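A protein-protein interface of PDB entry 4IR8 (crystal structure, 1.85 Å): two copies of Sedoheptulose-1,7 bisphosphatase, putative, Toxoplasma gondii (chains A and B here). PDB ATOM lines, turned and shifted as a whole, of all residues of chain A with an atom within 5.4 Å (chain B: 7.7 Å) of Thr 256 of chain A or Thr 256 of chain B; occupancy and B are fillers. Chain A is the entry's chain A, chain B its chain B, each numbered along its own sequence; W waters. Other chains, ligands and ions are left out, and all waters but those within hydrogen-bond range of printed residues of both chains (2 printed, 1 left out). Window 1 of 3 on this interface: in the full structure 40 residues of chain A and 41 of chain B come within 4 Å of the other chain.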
ATOM      1  N   ILE A 131      14.616 -19.945  24.908  1.00  0.00           N
ATOM      2  CA  ILE A 131      15.660 -20.615  24.103  1.00  0.00           C
ATOM      3  C   ILE A 131      17.081 -20.504  24.649  1.00  0.00           C
ATOM      4  O   ILE A 131      18.003 -21.169  24.156  1.00  0.00           O
ATOM      5  CB  ILE A 131      15.659 -20.111  22.626  1.00  0.00           C
ATOM      6  CG1 ILE A 131      15.980 -18.594  22.546  1.00  0.00           C
ATOM      7  CG2 ILE A 131      14.325 -20.474  21.942  1.00  0.00           C
ATOM      8  CD1 ILE A 131      16.108 -18.068  21.140  1.00  0.00           C
ATOM      9  N   TRP A 136      21.017 -21.169  22.028  1.00  0.00           N
ATOM     10  CA  TRP A 136      20.643 -20.492  20.810  1.00  0.00           C
ATOM     11  C   TRP A 136      20.957 -19.013  21.028  1.00  0.00           C
ATOM     12  O   TRP A 136      21.163 -18.574  22.145  1.00  0.00           O
ATOM     13  CB  TRP A 136      19.157 -20.716  20.542  1.00  0.00           C
ATOM     14  CG  TRP A 136      18.827 -22.086  19.998  1.00  0.00           C
ATOM     15  CD1 TRP A 136      19.592 -23.213  20.056  1.00  0.00           C
ATOM     16  CD2 TRP A 136      17.601 -22.467  19.385  1.00  0.00           C
ATOM     17  NE1 TRP A 136      18.919 -24.273  19.488  1.00  0.00           N
ATOM     18  CE2 TRP A 136      17.706 -23.832  19.039  1.00  0.00           C
ATOM     19  CE3 TRP A 136      16.428 -21.778  19.071  1.00  0.00           C
ATOM     20  CZ2 TRP A 136      16.667 -24.526  18.422  1.00  0.00           C
ATOM     21  CZ3 TRP A 136      15.409 -22.457  18.442  1.00  0.00           C
ATOM     22  CH2 TRP A 136      15.533 -23.822  18.120  1.00  0.00           C
ATOM     23  N   ALA A 137      21.046 -18.258  19.949  1.00  0.00           N
ATOM     24  CA  ALA A 137      21.344 -16.831  20.060  1.00  0.00           C
ATOM     25  C   ALA A 137      20.222 -16.089  20.799  1.00  0.00           C
ATOM     26  O   ALA A 137      19.056 -16.446  20.698  1.00  0.00           O
ATOM     27  CB  ALA A 137      21.585 -16.229  18.685  1.00  0.00           C
ATOM     28  N   SER A 226       9.257 -15.172   9.255  1.00  0.00           N
ATOM     29  CA  SER A 226       9.531 -15.511  10.636  1.00  0.00           C
ATOM     30  C   SER A 226       8.244 -15.243  11.421  1.00  0.00           C
ATOM     31  O   SER A 226       7.986 -14.125  11.839  1.00  0.00           O
ATOM     32  CB  SER A 226      10.713 -14.664  11.125  1.00  0.00           C
ATOM     33  OG  SER A 226      11.162 -15.067  12.404  1.00  0.00           O
ATOM     34  N   ARG A 254      12.431 -19.173   8.969  1.00  0.00           N
ATOM     35  CA  ARG A 254      13.538 -18.938   9.914  1.00  0.00           C
ATOM     36  C   ARG A 254      12.940 -18.287  11.139  1.00  0.00           C
ATOM     37  O   ARG A 254      12.577 -17.091  11.117  1.00  0.00           O
ATOM     38  CB  ARG A 254      14.627 -18.034   9.311  1.00  0.00           C
ATOM     39  CG  ARG A 254      15.372 -18.625   8.135  1.00  0.00           C
ATOM     40  CD  ARG A 254      16.316 -19.751   8.591  1.00  0.00           C
ATOM     41  NE  ARG A 254      17.098 -20.329   7.506  1.00  0.00           N
ATOM     42  CZ  ARG A 254      16.756 -21.406   6.797  1.00  0.00           C
ATOM     43  NH1 ARG A 254      15.607 -22.045   7.023  1.00  0.00           N
ATOM     44  NH2 ARG A 254      17.569 -21.846   5.848  1.00  0.00           N
ATOM     45  N   TYR A 255      12.826 -19.063  12.213  1.00  0.00           N
ATOM     46  CA  TYR A 255      12.158 -18.593  13.407  1.00  0.00           C
ATOM     47  C   TYR A 255      12.736 -19.245  14.652  1.00  0.00           C
ATOM     48  O   TYR A 255      12.425 -20.410  14.965  1.00  0.00           O
ATOM     49  CB  TYR A 255      10.639 -18.878  13.320  1.00  0.00           C
ATOM     50  CG  TYR A 255       9.985 -18.336  14.532  1.00  0.00           C
ATOM     51  CD1 TYR A 255       9.917 -16.966  14.734  1.00  0.00           C
ATOM     52  CD2 TYR A 255       9.516 -19.170  15.533  1.00  0.00           C
ATOM     53  CE1 TYR A 255       9.380 -16.447  15.864  1.00  0.00           C
ATOM     54  CE2 TYR A 255       8.976 -18.643  16.680  1.00  0.00           C
ATOM     55  CZ  TYR A 255       8.919 -17.283  16.839  1.00  0.00           C
ATOM     56  OH  TYR A 255       8.390 -16.730  17.971  1.00  0.00           O
ATOM     57  N   THR A 256      13.583 -18.504  15.369  1.00  0.00           N
ATOM     58  CA  THR A 256      14.245 -19.089  16.531  1.00  0.00           C
ATOM     59  C   THR A 256      13.442 -18.964  17.817  1.00  0.00           C
ATOM     60  O   THR A 256      13.680 -19.700  18.758  1.00  0.00           O
ATOM     61  CB  THR A 256      15.652 -18.466  16.784  1.00  0.00           C
ATOM     62  OG1 THR A 256      15.524 -17.170  17.373  1.00  0.00           O
ATOM     63  CG2 THR A 256      16.468 -18.374  15.500  1.00  0.00           C
ATOM     64  N   GLY A 257      12.508 -18.018  17.870  1.00  0.00           N
ATOM     65  CA  GLY A 257      11.777 -17.767  19.111  1.00  0.00           C
ATOM     66  C   GLY A 257      12.410 -16.671  19.964  1.00  0.00           C
ATOM     67  O   GLY A 257      11.869 -16.311  20.995  1.00  0.00           O
ATOM     68  N   GLY A 258      13.570 -16.180  19.552  1.00  0.00           N
ATOM     69  CA  GLY A 258      14.252 -15.071  20.216  1.00  0.00           C
ATOM     70  C   GLY A 258      14.025 -13.834  19.375  1.00  0.00           C
ATOM     71  O   GLY A 258      14.471 -13.765  18.227  1.00  0.00           O
ATOM     72  N   PRO A 261      17.374 -12.068  17.652  1.00  0.00           N
ATOM     73  CA  PRO A 261      17.942 -12.764  16.489  1.00  0.00           C
ATOM     74  C   PRO A 261      16.954 -12.899  15.346  1.00  0.00           C
ATOM     75  O   PRO A 261      17.358 -12.825  14.188  1.00  0.00           O
ATOM     76  CB  PRO A 261      18.359 -14.135  17.036  1.00  0.00           C
ATOM     77  CG  PRO A 261      17.928 -14.181  18.435  1.00  0.00           C
ATOM     78  CD  PRO A 261      17.528 -12.827  18.899  1.00  0.00           C
ATOM     79  N   ASP A 262      15.662 -13.054  15.660  1.00  0.00           N
ATOM     80  CA  ASP A 262      14.626 -13.189  14.625  1.00  0.00           C
ATOM     81  C   ASP A 262      14.468 -11.949  13.742  1.00  0.00           C
ATOM     82  O   ASP A 262      14.077 -12.067  12.589  1.00  0.00           O
ATOM     83  CB  ASP A 262      13.279 -13.579  15.247  1.00  0.00           C
ATOM     84  CG  ASP A 262      13.260 -15.019  15.755  1.00  0.00           C
ATOM     85  OD1 ASP A 262      14.149 -15.815  15.359  1.00  0.00           O
ATOM     86  OD2 ASP A 262      12.346 -15.352  16.523  1.00  0.00           O
ATOM     87  N   GLY B 128      25.440 -25.077   9.258  1.00  0.00           N
ATOM     88  CA  GLY B 128      24.575 -23.884   9.371  1.00  0.00           C
ATOM     89  C   GLY B 128      24.981 -22.750   8.444  1.00  0.00           C
ATOM     90  O   GLY B 128      24.968 -21.584   8.835  1.00  0.00           O
ATOM     91  N   SER B 130      23.546 -21.281   5.911  1.00  0.00           N
ATOM     92  CA  SER B 130      22.583 -20.238   5.578  1.00  0.00           C
ATOM     93  C   SER B 130      22.285 -19.275   6.725  1.00  0.00           C
ATOM     94  O   SER B 130      21.640 -18.261   6.481  1.00  0.00           O
ATOM     95  CB  SER B 130      21.255 -20.822   5.043  1.00  0.00           C
ATOM     96  OG  SER B 130      20.480 -21.425   6.072  1.00  0.00           O
ATOM     97  N   ILE B 131      22.778 -19.548   7.933  1.00  0.00           N
ATOM     98  CA  ILE B 131      22.479 -18.686   9.098  1.00  0.00           C
ATOM     99  C   ILE B 131      23.692 -18.199   9.870  1.00  0.00           C
ATOM    100  O   ILE B 131      23.537 -17.410  10.799  1.00  0.00           O
ATOM    101  CB  ILE B 131      21.523 -19.396  10.103  1.00  0.00           C
ATOM    102  CG1 ILE B 131      22.166 -20.651  10.708  1.00  0.00           C
ATOM    103  CG2 ILE B 131      20.226 -19.746   9.400  1.00  0.00           C
ATOM    104  CD1 ILE B 131      21.329 -21.337  11.806  1.00  0.00           C
ATOM    105  N   TRP B 136      23.498 -16.536  14.294  1.00  0.00           N
ATOM    106  CA  TRP B 136      22.691 -17.548  14.955  1.00  0.00           C
ATOM    107  C   TRP B 136      23.607 -18.715  15.340  1.00  0.00           C
ATOM    108  O   TRP B 136      24.707 -18.856  14.803  1.00  0.00           O
ATOM    109  CB  TRP B 136      21.582 -18.001  14.011  1.00  0.00           C
ATOM    110  CG  TRP B 136      20.490 -16.960  13.819  1.00  0.00           C
ATOM    111  CD1 TRP B 136      20.557 -15.623  14.125  1.00  0.00           C
ATOM    112  CD2 TRP B 136      19.205 -17.165  13.209  1.00  0.00           C
ATOM    113  NE1 TRP B 136      19.361 -15.006  13.818  1.00  0.00           N
ATOM    114  CE2 TRP B 136      18.527 -15.927  13.228  1.00  0.00           C
ATOM    115  CE3 TRP B 136      18.559 -18.280  12.645  1.00  0.00           C
ATOM    116  CZ2 TRP B 136      17.216 -15.780  12.749  1.00  0.00           C
ATOM    117  CZ3 TRP B 136      17.261 -18.130  12.163  1.00  0.00           C
ATOM    118  CH2 TRP B 136      16.603 -16.883  12.222  1.00  0.00           C
ATOM    119  N   ALA B 137      23.140 -19.540  16.276  1.00  0.00           N
ATOM    120  CA  ALA B 137      23.877 -20.709  16.732  1.00  0.00           C
ATOM    121  C   ALA B 137      24.081 -21.669  15.554  1.00  0.00           C
ATOM    122  O   ALA B 137      23.225 -21.772  14.682  1.00  0.00           O
ATOM    123  CB  ALA B 137      23.150 -21.386  17.875  1.00  0.00           C
ATOM    124  N   VAL B 138      25.274 -22.249  15.482  1.00  0.00           N
ATOM    125  CA  VAL B 138      25.633 -23.220  14.456  1.00  0.00           C
ATOM    126  C   VAL B 138      26.291 -24.380  15.184  1.00  0.00           C
ATOM    127  O   VAL B 138      26.198 -24.459  16.411  1.00  0.00           O
ATOM    128  CB  VAL B 138      26.514 -22.617  13.375  1.00  0.00           C
ATOM    129  CG1 VAL B 138      25.721 -21.573  12.574  1.00  0.00           C
ATOM    130  CG2 VAL B 138      27.787 -21.981  14.003  1.00  0.00           C
ATOM    131  N   SER B 226       9.836 -28.658  14.804  1.00  0.00           N
ATOM    132  CA  SER B 226      10.911 -28.029  14.041  1.00  0.00           C
ATOM    133  C   SER B 226      10.866 -28.622  12.625  1.00  0.00           C
ATOM    134  O   SER B 226      11.487 -29.656  12.343  1.00  0.00           O
ATOM    135  CB  SER B 226      12.249 -28.290  14.766  1.00  0.00           C
ATOM    136  OG  SER B 226      13.329 -27.498  14.258  1.00  0.00           O
ATOM    137  N   PRO B 227      10.107 -27.967  11.730  1.00  0.00           N
ATOM    138  CA  PRO B 227       9.876 -28.496  10.396  1.00  0.00           C
ATOM    139  C   PRO B 227      10.852 -28.010   9.340  1.00  0.00           C
ATOM    140  O   PRO B 227      10.691 -26.903   8.814  1.00  0.00           O
ATOM    141  CB  PRO B 227       8.464 -28.005  10.088  1.00  0.00           C
ATOM    142  CG  PRO B 227       8.386 -26.659  10.795  1.00  0.00           C
ATOM    143  CD  PRO B 227       9.317 -26.736  11.976  1.00  0.00           C
ATOM    144  N   THR B 252       4.741 -25.520  19.874  1.00  0.00           N
ATOM    145  CA  THR B 252       5.622 -24.366  19.767  1.00  0.00           C
ATOM    146  C   THR B 252       6.592 -24.533  18.589  1.00  0.00           C
ATOM    147  O   THR B 252       7.315 -25.527  18.501  1.00  0.00           O
ATOM    148  CB  THR B 252       6.402 -24.182  21.085  1.00  0.00           C
ATOM    149  OG1 THR B 252       5.467 -24.028  22.164  1.00  0.00           O
ATOM    150  CG2 THR B 252       7.326 -22.950  21.020  1.00  0.00           C
ATOM    151  N   LEU B 253       6.605 -23.563  17.684  1.00  0.00           N
ATOM    152  CA  LEU B 253       7.494 -23.616  16.528  1.00  0.00           C
ATOM    153  C   LEU B 253       8.899 -23.131  16.903  1.00  0.00           C
ATOM    154  O   LEU B 253       9.060 -22.024  17.399  1.00  0.00           O
ATOM    155  CB  LEU B 253       6.956 -22.724  15.402  1.00  0.00           C
ATOM    156  CG  LEU B 253       7.820 -22.587  14.147  1.00  0.00           C
ATOM    157  CD1 LEU B 253       8.025 -23.944  13.437  1.00  0.00           C
ATOM    158  CD2 LEU B 253       7.221 -21.541  13.190  1.00  0.00           C
ATOM    159  N   ARG B 254       9.911 -23.951  16.627  1.00  0.00           N
ATOM    160  CA  ARG B 254      11.315 -23.583  16.903  1.00  0.00           C
ATOM    161  C   ARG B 254      12.149 -24.167  15.783  1.00  0.00           C
ATOM    162  O   ARG B 254      12.411 -25.365  15.752  1.00  0.00           O
ATOM    163  CB  ARG B 254      11.775 -24.112  18.257  1.00  0.00           C
ATOM    164  CG  ARG B 254      11.103 -23.489  19.474  1.00  0.00           C
ATOM    165  CD  ARG B 254      11.559 -22.059  19.713  1.00  0.00           C
ATOM    166  NE  ARG B 254      10.942 -21.403  20.879  1.00  0.00           N
ATOM    167  CZ  ARG B 254       9.859 -20.643  20.849  1.00  0.00           C
ATOM    168  NH1 ARG B 254       9.189 -20.447  19.715  1.00  0.00           N
ATOM    169  NH2 ARG B 254       9.426 -20.072  21.966  1.00  0.00           N
ATOM    170  N   TYR B 255      12.557 -23.317  14.850  1.00  0.00           N
ATOM    171  CA  TYR B 255      13.274 -23.772  13.668  1.00  0.00           C
ATOM    172  C   TYR B 255      14.256 -22.712  13.171  1.00  0.00           C
ATOM    173  O   TYR B 255      13.867 -21.736  12.534  1.00  0.00           O
ATOM    174  CB  TYR B 255      12.270 -24.135  12.566  1.00  0.00           C
ATOM    175  CG  TYR B 255      12.982 -24.604  11.354  1.00  0.00           C
ATOM    176  CD1 TYR B 255      13.594 -25.846  11.342  1.00  0.00           C
ATOM    177  CD2 TYR B 255      13.131 -23.783  10.244  1.00  0.00           C
ATOM    178  CE1 TYR B 255      14.322 -26.269  10.254  1.00  0.00           C
ATOM    179  CE2 TYR B 255      13.857 -24.210   9.143  1.00  0.00           C
ATOM    180  CZ  TYR B 255      14.457 -25.452   9.167  1.00  0.00           C
ATOM    181  OH  TYR B 255      15.189 -25.906   8.099  1.00  0.00           O
ATOM    182  N   THR B 256      15.533 -22.929  13.464  1.00  0.00           N
ATOM    183  CA  THR B 256      16.573 -21.958  13.117  1.00  0.00           C
ATOM    184  C   THR B 256      17.175 -22.151  11.730  1.00  0.00           C
ATOM    185  O   THR B 256      17.764 -21.222  11.197  1.00  0.00           O
ATOM    186  CB  THR B 256      17.730 -21.982  14.110  1.00  0.00           C
ATOM    187  OG1 THR B 256      18.568 -23.121  13.854  1.00  0.00           O
ATOM    188  CG2 THR B 256      17.202 -22.004  15.575  1.00  0.00           C
ATOM    189  N   GLY B 257      17.041 -23.345  11.147  1.00  0.00           N
ATOM    190  CA  GLY B 257      17.639 -23.613   9.845  1.00  0.00           C
ATOM    191  C   GLY B 257      19.050 -24.203   9.969  1.00  0.00           C
ATOM    192  O   GLY B 257      19.711 -24.464   8.957  1.00  0.00           O
ATOM    193  N   GLY B 258      19.527 -24.352  11.207  1.00  0.00           N
ATOM    194  CA  GLY B 258      20.822 -24.978  11.505  1.00  0.00           C
ATOM    195  C   GLY B 258      20.505 -26.327  12.116  1.00  0.00           C
ATOM    196  O   GLY B 258      19.910 -26.404  13.188  1.00  0.00           O
ATOM    197  N   LEU B 259      20.903 -27.402  11.442  1.00  0.00           N
ATOM    198  CA  LEU B 259      20.594 -28.764  11.910  1.00  0.00           C
ATOM    199  C   LEU B 259      20.996 -29.052  13.362  1.00  0.00           C
ATOM    200  O   LEU B 259      20.204 -29.563  14.125  1.00  0.00           O
ATOM    201  CB  LEU B 259      21.260 -29.785  10.999  1.00  0.00           C
ATOM    202  CG  LEU B 259      21.003 -31.254  11.333  1.00  0.00           C
ATOM    203  CD1 LEU B 259      19.497 -31.620  11.283  1.00  0.00           C
ATOM    204  CD2 LEU B 259      21.858 -32.114  10.387  1.00  0.00           C
ATOM    205  N   VAL B 260      22.228 -28.714  13.740  1.00  0.00           N
ATOM    206  CA  VAL B 260      22.720 -28.999  15.081  1.00  0.00           C
ATOM    207  C   VAL B 260      21.913 -28.276  16.166  1.00  0.00           C
ATOM    208  O   VAL B 260      21.399 -28.941  17.063  1.00  0.00           O
ATOM    209  CB  VAL B 260      24.251 -28.750  15.230  1.00  0.00           C
ATOM    210  CG1 VAL B 260      24.687 -29.044  16.629  1.00  0.00           C
ATOM    211  CG2 VAL B 260      25.011 -29.637  14.263  1.00  0.00           C
ATOM    212  N   PRO B 261      21.756 -26.936  16.070  1.00  0.00           N
ATOM    213  CA  PRO B 261      20.917 -26.301  17.079  1.00  0.00           C
ATOM    214  C   PRO B 261      19.461 -26.816  17.066  1.00  0.00           C
ATOM    215  O   PRO B 261      18.840 -26.953  18.129  1.00  0.00           O
ATOM    216  CB  PRO B 261      20.939 -24.807  16.692  1.00  0.00           C
ATOM    217  CG  PRO B 261      21.607 -24.719  15.392  1.00  0.00           C
ATOM    218  CD  PRO B 261      22.476 -25.939  15.256  1.00  0.00           C
ATOM    219  N   ASP B 262      18.937 -27.096  15.872  1.00  0.00           N
ATOM    220  CA  ASP B 262      17.530 -27.525  15.747  1.00  0.00           C
ATOM    221  C   ASP B 262      17.268 -28.864  16.427  1.00  0.00           C
ATOM    222  O   ASP B 262      16.159 -29.110  16.896  1.00  0.00           O
ATOM    223  CB  ASP B 262      17.071 -27.537  14.291  1.00  0.00           C
ATOM    224  CG  ASP B 262      16.931 -26.145  13.701  1.00  0.00           C
ATOM    225  OD1 ASP B 262      16.787 -25.155  14.465  1.00  0.00           O
ATOM    226  OD2 ASP B 262      16.901 -26.049  12.449  1.00  0.00           O
ATOM    227  N   VAL B 263      18.270 -29.740  16.498  1.00  0.00           N
ATOM    228  CA  VAL B 263      18.073 -31.008  17.207  1.00  0.00           C
ATOM    229  C   VAL B 263      18.582 -30.923  18.643  1.00  0.00           C
ATOM    230  O   VAL B 263      18.052 -31.606  19.517  1.00  0.00           O
ATOM    231  CB  VAL B 263      18.650 -32.242  16.452  1.00  0.00           C
ATOM    232  CG1 VAL B 263      18.087 -32.289  15.033  1.00  0.00           C
ATOM    233  CG2 VAL B 263      20.167 -32.226  16.435  1.00  0.00           C
ATOM    234  N   GLN B 265      18.090 -28.592  20.810  1.00  0.00           N
ATOM    235  CA  GLN B 265      16.987 -28.148  21.664  1.00  0.00           C
ATOM    236  C   GLN B 265      16.166 -29.296  22.254  1.00  0.00           C
ATOM    237  O   GLN B 265      15.626 -29.172  23.350  1.00  0.00           O
ATOM    238  CB  GLN B 265      16.051 -27.200  20.912  1.00  0.00           C
ATOM    239  CG  GLN B 265      15.357 -27.831  19.729  1.00  0.00           C
ATOM    240  CD  GLN B 265      14.307 -26.954  19.116  1.00  0.00           C
ATOM    241  OE1 GLN B 265      13.636 -26.190  19.813  1.00  0.00           O
ATOM    242  NE2 GLN B 265      14.104 -27.100  17.811  1.00  0.00           N
ATOM    243  N   PHE B 274      11.857 -32.934  15.411  1.00  0.00           N
ATOM    244  CA  PHE B 274      12.519 -32.354  14.271  1.00  0.00           C
ATOM    245  C   PHE B 274      12.172 -33.213  13.073  1.00  0.00           C
ATOM    246  O   PHE B 274      12.283 -34.449  13.139  1.00  0.00           O
ATOM    247  CB  PHE B 274      14.043 -32.325  14.474  1.00  0.00           C
ATOM    248  CG  PHE B 274      14.791 -31.955  13.248  1.00  0.00           C
ATOM    249  CD1 PHE B 274      15.000 -30.619  12.924  1.00  0.00           C
ATOM    250  CD2 PHE B 274      15.251 -32.934  12.378  1.00  0.00           C
ATOM    251  CE1 PHE B 274      15.660 -30.274  11.759  1.00  0.00           C
ATOM    252  CE2 PHE B 274      15.912 -32.575  11.202  1.00  0.00           C
ATOM    253  CZ  PHE B 274      16.124 -31.247  10.914  1.00  0.00           C
HETATM  254  O   HOH W   1      18.863 -18.044   6.640  1.00  0.00           O
HETATM  255  O   HOH W   2      20.292 -19.341  17.271  1.00  0.00           O
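The backbone carbonyl oxygen (O) of Arg 254 of chain A lies within hydrogen-bond range of the side-chain hydroxyl (OG) of Ser 226 of chain A (2.8 Å). OG1 of Thr 256 of chain A sits at hydrogen-bond distance from N of Gly 258 of chain A, at 3.1 Å. N of Thr 256 of chain A lies within hydrogen-bond range of OD1 of Asp 262 of chain A (2.7 Å). The backbone carbonyl oxygen (O) of Arg 254 of chain B is in hydrogen-bond range of the side-chain amide nitrogen (NE2) of Gln 265 of chain B (3.2 Å). N of Gly 258 of chain B lies within hydrogen-bond range of OG1 of Thr 256 of chain B (3.1 Å). The side-chain carboxylate (OD2) of Asp 262 of chain B sits at hydrogen-bond distance from the backbone NH (N) of Gly 257 of chain B (3.0 Å).
Water W1 lies within hydrogen-bond range of the backbone carbonyl oxygen (O) of Ser 130 of chain B and the guanidinium group (NE) of Arg 254 of chain A. Water W2 bridges N of Ala 137 of chain A (3.0 Å) and N of Ala 137 of chain B (3.0 Å).
Hydrophobic or aromatic side chains of chain B within 4 Å of the printed part of chain A: Ile 131, Trp 136, Ala 137, Tyr 255 and Pro 261. Hydrophobic or aromatic side chains of chain A within 4 Å of the printed part of chain B: Ile 131, Trp 136, Tyr 255 and Pro 261. Among the printed residues, 20 pairs touch across the chains.
Of the printed residues of chain B, Tyr 255 of chain A touches Leu 253 (3.4 Å), Arg 254 (3.5 Å) and Tyr 255 (2.9 Å). Of the printed residues of chain B, Gly 257 of chain A touches Arg 254 (3.8 Å). Of the printed residues of chain A, Trp 136 of chain B touches Arg 254 (3.7 Å), Thr 256 (3.4 Å) and Pro 261 (3.0 Å). Of the printed residues of chain A, Thr 256 of chain B touches Trp 136 (3.4 Å), Arg 254 (3.3 Å) and Thr 256 (3.7 Å). Printed residues of chain A within 4 Å of Gly 257 of chain B: Arg 254. Phe 274 of chain B touches none of the printed residues of chain A. The nearest residue of chain B that does not touch Thr 256 of chain A is Tyr 255 of chain B (4.3 Å).
Arg 254 of chain B touches Ile 131 of chain A. CA of Trp 136 of chain A touches CB of Ala 137 of chain B, at 3.96 Å. Ile 131 of chain B touches Arg 254 of chain A (CG2 to NE, 3.7 Å). Trp 136 of chain B touches Arg 254 of chain A (CH2 to CB, 3.7 Å). Arg 254 of chain A touches Tyr 255 of chain B. Arg 254 of chain A touches Gly 257 of chain B. Tyr 255 of chain A touches Arg 254 of chain B. Thr 256 of chain A touches Trp 136 of chain B. Thr 256 of chain B touches Thr 256 of chain A. Gly 257 of chain A touches Arg 254 of chain B.
The indole nitrogen of Trp 136 of chain A is in hydrogen-bond range of the backbone carbonyl oxygen of Pro 261 of chain B, at 3.0 Å. The side-chain hydroxyl of Ser 130 of chain B sits at hydrogen-bond distance from the guanidinium group of Arg 254 of chain A. N of Tyr 255 of chain A is in hydrogen-bond range of O of Tyr 255 of chain B. The indole nitrogen (NE1) of Trp 136 of chain B is in hydrogen-bond range of the backbone carbonyl oxygen (O) of Pro 261 of chain A (3.0 Å).
Trp 136 of chain A touches Pro 261 of chain B, and with the chains exchanged Pro 261 of chain A touches Trp 136 of chain B. Arg 254 of chain A touches Thr 256 of chain B, and with the chains exchanged Thr 256 of chain A touches Arg 254 of chain B. Arg 254 of chain A touches Gly 257 of chain B, and with the chains exchanged Gly 257 of chain A touches Arg 254 of chain B. Thr 256 of chain A touches its own counterpart, Thr 256 of chain B. Positions printed for both chains: 131, 136, 137, 226, 254, 255, 256, 257, 258, 261 and 262. Of the 20 pairs that touch across the chains among the printed residues, 16 have their exchanged pair printed and touching as well.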
